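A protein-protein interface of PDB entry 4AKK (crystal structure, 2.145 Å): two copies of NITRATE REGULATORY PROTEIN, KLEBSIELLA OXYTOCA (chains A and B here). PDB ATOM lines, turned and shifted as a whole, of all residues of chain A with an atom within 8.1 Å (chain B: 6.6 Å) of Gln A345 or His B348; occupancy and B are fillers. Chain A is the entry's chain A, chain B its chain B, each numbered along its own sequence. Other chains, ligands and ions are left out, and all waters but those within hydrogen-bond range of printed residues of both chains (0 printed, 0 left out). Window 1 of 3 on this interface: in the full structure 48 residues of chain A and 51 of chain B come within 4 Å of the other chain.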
ATOM      1  N   VAL A 187      16.260 -20.521   6.207  1.00  0.00           N
ATOM      2  CA  VAL A 187      17.158 -21.350   5.414  1.00  0.00           C
ATOM      3  C   VAL A 187      16.400 -22.177   4.367  1.00  0.00           C
ATOM      4  O   VAL A 187      16.844 -22.299   3.224  1.00  0.00           O
ATOM      5  CB  VAL A 187      18.037 -22.250   6.305  1.00  0.00           C
ATOM      6  CG1 VAL A 187      18.728 -23.330   5.470  1.00  0.00           C
ATOM      7  CG2 VAL A 187      19.065 -21.402   7.027  1.00  0.00           C
ATOM      8  N   SER A 236      17.797 -29.503   0.291  1.00  0.00           N
ATOM      9  CA  SER A 236      17.827 -28.720   1.513  1.00  0.00           C
ATOM     10  C   SER A 236      16.436 -28.156   1.860  1.00  0.00           C
ATOM     11  O   SER A 236      15.998 -28.245   3.012  1.00  0.00           O
ATOM     12  CB  SER A 236      18.880 -27.617   1.432  1.00  0.00           C
ATOM     13  OG  SER A 236      18.745 -26.727   2.523  1.00  0.00           O
ATOM     14  N   LEU A 339      20.624 -24.089  18.448  1.00  0.00           N
ATOM     15  CA  LEU A 339      21.592 -23.472  17.542  1.00  0.00           C
ATOM     16  C   LEU A 339      21.460 -23.961  16.091  1.00  0.00           C
ATOM     17  O   LEU A 339      21.754 -23.222  15.153  1.00  0.00           O
ATOM     18  CB  LEU A 339      23.028 -23.683  18.050  1.00  0.00           C
ATOM     19  CG  LEU A 339      23.329 -23.195  19.473  1.00  0.00           C
ATOM     20  CD1 LEU A 339      24.821 -23.223  19.738  1.00  0.00           C
ATOM     21  CD2 LEU A 339      22.780 -21.795  19.708  1.00  0.00           C
ATOM     22  N   LEU A 340      21.028 -25.205  15.916  1.00  0.00           N
ATOM     23  CA  LEU A 340      20.816 -25.764  14.585  1.00  0.00           C
ATOM     24  C   LEU A 340      22.070 -25.695  13.717  1.00  0.00           C
ATOM     25  O   LEU A 340      22.076 -25.043  12.667  1.00  0.00           O
ATOM     26  CB  LEU A 340      19.680 -25.032  13.894  1.00  0.00           C
ATOM     27  CG  LEU A 340      18.313 -25.252  14.525  1.00  0.00           C
ATOM     28  CD1 LEU A 340      17.272 -24.442  13.768  1.00  0.00           C
ATOM     29  CD2 LEU A 340      17.984 -26.731  14.503  1.00  0.00           C
ATOM     30  N   PRO A 341      23.139 -26.373  14.145  1.00  0.00           N
ATOM     31  CA  PRO A 341      24.398 -26.323  13.391  1.00  0.00           C
ATOM     32  C   PRO A 341      24.241 -26.904  11.983  1.00  0.00           C
ATOM     33  O   PRO A 341      24.790 -26.345  11.044  1.00  0.00           O
ATOM     34  CB  PRO A 341      25.347 -27.185  14.241  1.00  0.00           C
ATOM     35  CG  PRO A 341      24.416 -28.069  15.046  1.00  0.00           C
ATOM     36  CD  PRO A 341      23.272 -27.163  15.379  1.00  0.00           C
ATOM     37  N   LEU A 342      23.491 -27.995  11.839  1.00  0.00           N
ATOM     38  CA  LEU A 342      23.269 -28.586  10.523  1.00  0.00           C
ATOM     39  C   LEU A 342      22.591 -27.603   9.577  1.00  0.00           C
ATOM     40  O   LEU A 342      22.902 -27.569   8.392  1.00  0.00           O
ATOM     41  CB  LEU A 342      22.437 -29.863  10.620  1.00  0.00           C
ATOM     42  CG  LEU A 342      23.015 -30.975  11.496  1.00  0.00           C
ATOM     43  CD1 LEU A 342      22.180 -32.245  11.374  1.00  0.00           C
ATOM     44  CD2 LEU A 342      24.466 -31.242  11.133  1.00  0.00           C
ATOM     45  N   VAL A 343      21.668 -26.805  10.108  1.00  0.00           N
ATOM     46  CA  VAL A 343      20.953 -25.824   9.299  1.00  0.00           C
ATOM     47  C   VAL A 343      21.885 -24.722   8.805  1.00  0.00           C
ATOM     48  O   VAL A 343      21.835 -24.336   7.643  1.00  0.00           O
ATOM     49  CB  VAL A 343      19.778 -25.189  10.070  1.00  0.00           C
ATOM     50  CG1 VAL A 343      19.239 -23.991   9.319  1.00  0.00           C
ATOM     51  CG2 VAL A 343      18.676 -26.208  10.290  1.00  0.00           C
ATOM     52  N   ARG A 344      22.730 -24.212   9.693  1.00  0.00           N
ATOM     53  CA  ARG A 344      23.711 -23.204   9.304  1.00  0.00           C
ATOM     54  C   ARG A 344      24.695 -23.779   8.278  1.00  0.00           C
ATOM     55  O   ARG A 344      25.109 -23.092   7.348  1.00  0.00           O
ATOM     56  CB  ARG A 344      24.460 -22.679  10.530  1.00  0.00           C
ATOM     57  CG  ARG A 344      23.563 -22.029  11.589  1.00  0.00           C
ATOM     58  CD  ARG A 344      22.468 -21.164  10.961  1.00  0.00           C
ATOM     59  NE  ARG A 344      21.979 -20.129  11.873  1.00  0.00           N
ATOM     60  CZ  ARG A 344      21.071 -20.329  12.825  1.00  0.00           C
ATOM     61  NH1 ARG A 344      20.549 -21.537  13.005  1.00  0.00           N
ATOM     62  NH2 ARG A 344      20.687 -19.323  13.603  1.00  0.00           N
ATOM     63  N   GLN A 345      25.052 -25.048   8.450  1.00  0.00           N
ATOM     64  CA  GLN A 345      25.928 -25.734   7.504  1.00  0.00           C
ATOM     65  C   GLN A 345      25.321 -25.764   6.104  1.00  0.00           C
ATOM     66  O   GLN A 345      26.012 -25.529   5.117  1.00  0.00           O
ATOM     67  CB  GLN A 345      26.218 -27.164   7.971  1.00  0.00           C
ATOM     68  CG  GLN A 345      27.082 -27.968   7.012  1.00  0.00           C
ATOM     69  CD  GLN A 345      28.492 -27.414   6.903  1.00  0.00           C
ATOM     70  OE1 GLN A 345      29.069 -26.958   7.894  1.00  0.00           O
ATOM     71  NE2 GLN A 345      29.054 -27.445   5.697  1.00  0.00           N
ATOM     72  N   GLN A 346      24.026 -26.057   6.024  1.00  0.00           N
ATOM     73  CA  GLN A 346      23.337 -26.114   4.739  1.00  0.00           C
ATOM     74  C   GLN A 346      23.334 -24.755   4.039  1.00  0.00           C
ATOM     75  O   GLN A 346      23.617 -24.662   2.846  1.00  0.00           O
ATOM     76  CB  GLN A 346      21.909 -26.622   4.928  1.00  0.00           C
ATOM     77  CG  GLN A 346      21.845 -28.068   5.378  1.00  0.00           C
ATOM     78  CD  GLN A 346      22.162 -29.030   4.250  1.00  0.00           C
ATOM     79  OE1 GLN A 346      21.333 -29.009   3.209  1.00  0.00           O
ATOM     80  NE2 GLN A 346      23.146 -29.778   4.306  1.00  0.00           N
ATOM     81  N   ALA A 347      23.011 -23.706   4.787  1.00  0.00           N
ATOM     82  CA  ALA A 347      23.090 -22.354   4.266  1.00  0.00           C
ATOM     83  C   ALA A 347      24.513 -22.020   3.782  1.00  0.00           C
ATOM     84  O   ALA A 347      24.670 -21.413   2.719  1.00  0.00           O
ATOM     85  CB  ALA A 347      22.598 -21.345   5.300  1.00  0.00           C
ATOM     86  N   HIS A 348      25.531 -22.432   4.545  1.00  0.00           N
ATOM     87  CA  HIS A 348      26.932 -22.252   4.143  1.00  0.00           C
ATOM     88  C   HIS A 348      27.192 -22.885   2.781  1.00  0.00           C
ATOM     89  O   HIS A 348      27.720 -22.250   1.877  1.00  0.00           O
ATOM     90  CB  HIS A 348      27.905 -22.934   5.123  1.00  0.00           C
ATOM     91  CG  HIS A 348      28.109 -22.211   6.418  1.00  0.00           C
ATOM     92  ND1 HIS A 348      28.124 -22.667   7.694  1.00  0.00           N
ATOM     93  CD2 HIS A 348      28.398 -20.865   6.490  1.00  0.00           C
ATOM     94  CE1 HIS A 348      28.395 -21.594   8.507  1.00  0.00           C
ATOM     95  NE2 HIS A 348      28.552 -20.518   7.757  1.00  0.00           N
ATOM     96  N   GLU A 349      26.862 -24.167   2.666  1.00  0.00           N
ATOM     97  CA  GLU A 349      27.138 -24.911   1.455  1.00  0.00           C
ATOM     98  C   GLU A 349      26.429 -24.311   0.234  1.00  0.00           C
ATOM     99  O   GLU A 349      26.985 -24.319  -0.864  1.00  0.00           O
ATOM    100  CB  GLU A 349      26.771 -26.388   1.626  1.00  0.00           C
ATOM    101  CG  GLU A 349      27.706 -27.173   2.533  1.00  0.00           C
ATOM    102  CD  GLU A 349      27.128 -28.524   2.931  1.00  0.00           C
ATOM    103  OE1 GLU A 349      25.902 -28.721   2.765  1.00  0.00           O
ATOM    104  OE2 GLU A 349      27.894 -29.389   3.414  1.00  0.00           O
ATOM    105  N   LEU A 350      25.218 -23.784   0.410  1.00  0.00           N
ATOM    106  CA  LEU A 350      24.471 -23.288  -0.749  1.00  0.00           C
ATOM    107  C   LEU A 350      25.059 -21.974  -1.248  1.00  0.00           C
ATOM    108  O   LEU A 350      25.123 -21.722  -2.456  1.00  0.00           O
ATOM    109  CB  LEU A 350      22.981 -23.146  -0.444  1.00  0.00           C
ATOM    110  CG  LEU A 350      22.288 -24.478  -0.136  1.00  0.00           C
ATOM    111  CD1 LEU A 350      20.792 -24.275  -0.095  1.00  0.00           C
ATOM    112  CD2 LEU A 350      22.670 -25.558  -1.151  1.00  0.00           C
ATOM    113  N   GLN A 351      25.492 -21.146  -0.304  1.00  0.00           N
ATOM    114  CA  GLN A 351      26.241 -19.935  -0.615  1.00  0.00           C
ATOM    115  C   GLN A 351      27.572 -20.274  -1.283  1.00  0.00           C
ATOM    116  O   GLN A 351      28.010 -19.590  -2.184  1.00  0.00           O
ATOM    117  CB  GLN A 351      26.509 -19.151   0.666  1.00  0.00           C
ATOM    118  CG  GLN A 351      25.333 -18.323   1.129  1.00  0.00           C
ATOM    119  CD  GLN A 351      25.388 -16.916   0.578  1.00  0.00           C
ATOM    120  OE1 GLN A 351      26.184 -16.094   1.031  1.00  0.00           O
ATOM    121  NE2 GLN A 351      24.539 -16.629  -0.406  1.00  0.00           N
ATOM    122  N   GLN A 352      28.214 -21.334  -0.817  1.00  0.00           N
ATOM    123  CA  GLN A 352      29.485 -21.760  -1.385  1.00  0.00           C
ATOM    124  C   GLN A 352      29.283 -22.170  -2.847  1.00  0.00           C
ATOM    125  O   GLN A 352      30.013 -21.736  -3.738  1.00  0.00           O
ATOM    126  CB  GLN A 352      30.057 -22.916  -0.562  1.00  0.00           C
ATOM    127  CG  GLN A 352      31.410 -23.423  -1.028  1.00  0.00           C
ATOM    128  CD  GLN A 352      31.967 -24.512  -0.128  1.00  0.00           C
ATOM    129  OE1 GLN A 352      31.219 -25.201   0.570  1.00  0.00           O
ATOM    130  NE2 GLN A 352      33.289 -24.675  -0.138  1.00  0.00           N
ATOM    131  N   ARG B 127      26.535 -21.584  24.518  1.00  0.00           N
ATOM    132  CA  ARG B 127      27.765 -22.370  24.497  1.00  0.00           C
ATOM    133  C   ARG B 127      28.485 -22.313  25.842  1.00  0.00           C
ATOM    134  O   ARG B 127      28.934 -23.330  26.368  1.00  0.00           O
ATOM    135  CB  ARG B 127      28.691 -21.878  23.380  1.00  0.00           C
ATOM    136  CG  ARG B 127      28.179 -22.157  21.979  1.00  0.00           C
ATOM    137  CD  ARG B 127      28.283 -23.636  21.629  1.00  0.00           C
ATOM    138  NE  ARG B 127      28.017 -23.869  20.212  1.00  0.00           N
ATOM    139  CZ  ARG B 127      27.741 -25.059  19.688  1.00  0.00           C
ATOM    140  NH1 ARG B 127      27.694 -26.136  20.463  1.00  0.00           N
ATOM    141  NH2 ARG B 127      27.501 -25.172  18.388  1.00  0.00           N
ATOM    142  N   PRO B 171      34.551 -21.213  18.184  1.00  0.00           N
ATOM    143  CA  PRO B 171      33.982 -20.812  16.895  1.00  0.00           C
ATOM    144  C   PRO B 171      32.859 -19.800  17.099  1.00  0.00           C
ATOM    145  O   PRO B 171      32.683 -18.878  16.297  1.00  0.00           O
ATOM    146  CB  PRO B 171      33.413 -22.125  16.333  1.00  0.00           C
ATOM    147  CG  PRO B 171      34.142 -23.210  17.067  1.00  0.00           C
ATOM    148  CD  PRO B 171      34.401 -22.658  18.432  1.00  0.00           C
ATOM    149  N   TYR B 190      41.711 -22.336  16.505  1.00  0.00           N
ATOM    150  CA  TYR B 190      40.728 -23.350  16.833  1.00  0.00           C
ATOM    151  C   TYR B 190      41.027 -24.651  16.088  1.00  0.00           C
ATOM    152  O   TYR B 190      40.929 -25.728  16.657  1.00  0.00           O
ATOM    153  CB  TYR B 190      39.323 -22.859  16.478  1.00  0.00           C
ATOM    154  CG  TYR B 190      38.287 -23.951  16.537  1.00  0.00           C
ATOM    155  CD1 TYR B 190      37.891 -24.493  17.756  1.00  0.00           C
ATOM    156  CD2 TYR B 190      37.723 -24.458  15.377  1.00  0.00           C
ATOM    157  CE1 TYR B 190      36.953 -25.504  17.816  1.00  0.00           C
ATOM    158  CE2 TYR B 190      36.778 -25.467  15.426  1.00  0.00           C
ATOM    159  CZ  TYR B 190      36.401 -25.988  16.647  1.00  0.00           C
ATOM    160  OH  TYR B 190      35.465 -26.988  16.691  1.00  0.00           O
ATOM    161  N   VAL B 343      36.280 -19.280   5.310  1.00  0.00           N
ATOM    162  CA  VAL B 343      37.062 -19.504   6.518  1.00  0.00           C
ATOM    163  C   VAL B 343      36.152 -19.834   7.698  1.00  0.00           C
ATOM    164  O   VAL B 343      36.397 -20.789   8.436  1.00  0.00           O
ATOM    165  CB  VAL B 343      37.938 -18.285   6.851  1.00  0.00           C
ATOM    166  CG1 VAL B 343      38.512 -18.402   8.237  1.00  0.00           C
ATOM    167  CG2 VAL B 343      39.038 -18.155   5.834  1.00  0.00           C
ATOM    168  N   ARG B 344      35.091 -19.057   7.875  1.00  0.00           N
ATOM    169  CA  ARG B 344      34.189 -19.304   8.992  1.00  0.00           C
ATOM    170  C   ARG B 344      33.423 -20.618   8.811  1.00  0.00           C
ATOM    171  O   ARG B 344      33.121 -21.312   9.777  1.00  0.00           O
ATOM    172  CB  ARG B 344      33.254 -18.113   9.240  1.00  0.00           C
ATOM    173  CG  ARG B 344      33.976 -16.889   9.836  1.00  0.00           C
ATOM    174  CD  ARG B 344      33.088 -16.146  10.847  1.00  0.00           C
ATOM    175  NE  ARG B 344      33.718 -14.936  11.386  1.00  0.00           N
ATOM    176  CZ  ARG B 344      33.970 -13.853  10.661  1.00  0.00           C
ATOM    177  NH1 ARG B 344      33.665 -13.844   9.375  1.00  0.00           N
ATOM    178  NH2 ARG B 344      34.535 -12.785  11.207  1.00  0.00           N
ATOM    179  N   GLN B 345      33.142 -20.974   7.568  1.00  0.00           N
ATOM    180  CA  GLN B 345      32.616 -22.297   7.277  1.00  0.00           C
ATOM    181  C   GLN B 345      33.568 -23.397   7.771  1.00  0.00           C
ATOM    182  O   GLN B 345      33.136 -24.327   8.446  1.00  0.00           O
ATOM    183  CB  GLN B 345      32.355 -22.456   5.781  1.00  0.00           C
ATOM    184  CG  GLN B 345      31.695 -23.770   5.411  1.00  0.00           C
ATOM    185  CD  GLN B 345      31.422 -23.884   3.921  1.00  0.00           C
ATOM    186  OE1 GLN B 345      31.081 -22.762   3.287  1.00  0.00           O
ATOM    187  NE2 GLN B 345      31.523 -24.967   3.346  1.00  0.00           N
ATOM    188  N   GLN B 346      34.854 -23.292   7.437  1.00  0.00           N
ATOM    189  CA  GLN B 346      35.849 -24.258   7.911  1.00  0.00           C
ATOM    190  C   GLN B 346      35.757 -24.482   9.416  1.00  0.00           C
ATOM    191  O   GLN B 346      35.806 -25.619   9.884  1.00  0.00           O
ATOM    192  CB  GLN B 346      37.269 -23.831   7.546  1.00  0.00           C
ATOM    193  CG  GLN B 346      37.598 -24.014   6.076  1.00  0.00           C
ATOM    194  CD  GLN B 346      39.056 -24.366   5.838  1.00  0.00           C
ATOM    195  OE1 GLN B 346      39.361 -25.404   5.248  1.00  0.00           O
ATOM    196  NE2 GLN B 346      39.964 -23.512   6.305  1.00  0.00           N
ATOM    197  N   ALA B 347      35.613 -23.397  10.168  1.00  0.00           N
ATOM    198  CA  ALA B 347      35.460 -23.485  11.615  1.00  0.00           C
ATOM    199  C   ALA B 347      34.231 -24.318  11.984  1.00  0.00           C
ATOM    200  O   ALA B 347      34.265 -25.140  12.910  1.00  0.00           O
ATOM    201  CB  ALA B 347      35.352 -22.096  12.212  1.00  0.00           C
ATOM    202  N   HIS B 348      33.143 -24.106  11.250  1.00  0.00           N
ATOM    203  CA  HIS B 348      31.906 -24.812  11.532  1.00  0.00           C
ATOM    204  C   HIS B 348      32.029 -26.286  11.160  1.00  0.00           C
ATOM    205  O   HIS B 348      31.520 -27.157  11.867  1.00  0.00           O
ATOM    206  CB  HIS B 348      30.733 -24.175  10.796  1.00  0.00           C
ATOM    207  CG  HIS B 348      29.407 -24.750  11.180  1.00  0.00           C
ATOM    208  ND1 HIS B 348      28.690 -25.772  10.653  1.00  0.00           N
ATOM    209  CD2 HIS B 348      28.673 -24.280  12.249  1.00  0.00           C
ATOM    210  CE1 HIS B 348      27.543 -25.891  11.399  1.00  0.00           C
ATOM    211  NE2 HIS B 348      27.557 -24.978  12.355  1.00  0.00           N
ATOM    212  N   GLU B 349      32.711 -26.562  10.054  1.00  0.00           N
ATOM    213  CA  GLU B 349      32.947 -27.937   9.642  1.00  0.00           C
ATOM    214  C   GLU B 349      33.771 -28.736  10.657  1.00  0.00           C
ATOM    215  O   GLU B 349      33.446 -29.885  10.937  1.00  0.00           O
ATOM    216  CB  GLU B 349      33.612 -27.990   8.269  1.00  0.00           C
ATOM    217  CG  GLU B 349      32.650 -27.736   7.117  1.00  0.00           C
ATOM    218  CD  GLU B 349      33.309 -27.862   5.751  1.00  0.00           C
ATOM    219  OE1 GLU B 349      34.553 -27.978   5.688  1.00  0.00           O
ATOM    220  OE2 GLU B 349      32.576 -27.842   4.737  1.00  0.00           O
ATOM    221  N   LEU B 350      34.834 -28.143  11.199  1.00  0.00           N
ATOM    222  CA  LEU B 350      35.657 -28.853  12.173  1.00  0.00           C
ATOM    223  C   LEU B 350      34.852 -29.106  13.441  1.00  0.00           C
ATOM    224  O   LEU B 350      34.894 -30.194  14.002  1.00  0.00           O
ATOM    225  CB  LEU B 350      36.954 -28.092  12.485  1.00  0.00           C
ATOM    226  CG  LEU B 350      37.929 -27.976  11.300  1.00  0.00           C
ATOM    227  CD1 LEU B 350      39.206 -27.250  11.700  1.00  0.00           C
ATOM    228  CD2 LEU B 350      38.241 -29.349  10.692  1.00  0.00           C
ATOM    229  N   GLN B 351      34.118 -28.093  13.886  1.00  0.00           N
ATOM    230  CA  GLN B 351      33.221 -28.237  15.023  1.00  0.00           C
ATOM    231  C   GLN B 351      32.225 -29.376  14.782  1.00  0.00           C
ATOM    232  O   GLN B 351      31.950 -30.171  15.666  1.00  0.00           O
ATOM    233  CB  GLN B 351      32.465 -26.927  15.259  1.00  0.00           C
ATOM    234  CG  GLN B 351      31.476 -26.987  16.401  1.00  0.00           C
ATOM    235  CD  GLN B 351      30.712 -25.693  16.555  1.00  0.00           C
ATOM    236  OE1 GLN B 351      29.793 -25.398  15.781  1.00  0.00           O
ATOM    237  NE2 GLN B 351      31.083 -24.909  17.558  1.00  0.00           N
ATOM    238  N   GLN B 352      31.691 -29.447  13.574  1.00  0.00           N
ATOM    239  CA  GLN B 352      30.771 -30.514  13.207  1.00  0.00           C
ATOM    240  C   GLN B 352      31.452 -31.886  13.192  1.00  0.00           C
ATOM    241  O   GLN B 352      30.877 -32.867  13.667  1.00  0.00           O
ATOM    242  CB  GLN B 352      30.111 -30.210  11.852  1.00  0.00           C
ATOM    243  CG  GLN B 352      29.676 -31.443  11.071  1.00  0.00           C
ATOM    244  CD  GLN B 352      29.647 -31.220   9.562  1.00  0.00           C
ATOM    245  OE1 GLN B 352      29.667 -30.082   9.088  1.00  0.00           O
ATOM    246  NE2 GLN B 352      29.599 -32.312   8.803  1.00  0.00           N
ATOM    247  N   LEU B 353      32.669 -31.958  12.650  1.00  0.00           N
ATOM    248  CA  LEU B 353      33.426 -33.208  12.630  1.00  0.00           C
ATOM    249  C   LEU B 353      33.598 -33.713  14.060  1.00  0.00           C
ATOM    250  O   LEU B 353      33.441 -34.902  14.336  1.00  0.00           O
ATOM    251  CB  LEU B 353      34.797 -33.026  11.955  1.00  0.00           C
ATOM    252  CG  LEU B 353      35.881 -34.085  12.259  1.00  0.00           C
ATOM    253  CD1 LEU B 353      35.493 -35.472  11.731  1.00  0.00           C
ATOM    254  CD2 LEU B 353      37.303 -33.672  11.760  1.00  0.00           C
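Among the printed residues, pairs that only touch across the chains: Leu A339 with Arg B127 (3.3 Å), Gln A345 with Glu B349 (3.7 Å) and His A348 with Gln B345 (3.7 Å).
Of the printed residues of chain A, His B348 touches Pro A341 (2.8 Å) and Gln A345 (3.0 Å).
No residue of chain A comes within 4 Å of Ala B347.
Printed residues of chain A within 4 Å of Arg B127: Leu A339.
Printed residues of chain B within 4 Å of Gln A352: Gln B345 (2.8 Å).
Of the printed residues of chain A, Gln B345 touches His A348 (3.7 Å) and Gln A352 (2.8 Å).
Printed residues of chain A within 4 Å of Glu B349: Gln A345 (3.7 Å).
Leu A340 touches none of the printed residues of chain B.
Ser A236 touches none of the printed residues of chain B.
The nearest residue of chain B that does not touch Gln A345 is Gln B345 (4.2 Å).
The nearest residue of chain A that does not touch His B348 is His A348 (4.2 Å).
The side-chain amide oxygen (OE1) of Gln A345 lies within hydrogen-bond range of a ring nitrogen (ND1) of His B348, 3.0 Å away.
OE1 of Gln B352 sits close to OE1 of Gln A345 (3.4 Å).
The side-chain amide oxygen (OE1) of Gln A352 lies within hydrogen-bond range of the side-chain amide nitrogen (NE2) of Gln B345 (2.8 Å).
A ring nitrogen (NE2) of His B348 lies close to the backbone carbonyl oxygen (O) of Pro A341.
Gln A345 touches His B348, and with the chains exchanged His A348 touches Gln B345.
Gln A345 touches Glu B349, but with the chains exchanged Glu A349 does not touch Gln B345 (4.5 Å).
Gln A345 touches Gln B352, and with the chains exchanged Gln A352 touches Gln B345.
Of the 7 pairs that touch across the chains among the printed residues, 4 have their exchanged pair printed and touching as well.
The side-chain carboxylate (OE2) of Glu A349 sits at hydrogen-bond distance from the side-chain amide nitrogen (NE2) of Gln A345, at 3.2 Å.
O of Leu A339 lies within hydrogen-bond range of NH1 of Arg A344 (3.0 Å).
The guanidinium group (NH2) of Arg B127 lies within hydrogen-bond range of the side-chain amide oxygen (OE1) of Gln B351 (3.5 Å).
The side-chain amide nitrogen (NE2) of Gln B345 lies within hydrogen-bond range of the side-chain carboxylate (OE2) of Glu B349 (3.4 Å).
A ring nitrogen (ND1) of His A348 lies within hydrogen-bond range of the backbone carbonyl oxygen (O) of Arg A344.
Hydrophobic or aromatic side chains of chain A that line the printed part of chain B: Leu A339, Pro A341 and His A348.
Among the printed residues, 7 pairs touch across the chains.
Among the printed residues, no Asp or Glu carboxylate lies within 4 Å of a Lys or Arg side-chain nitrogen of the other chain.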
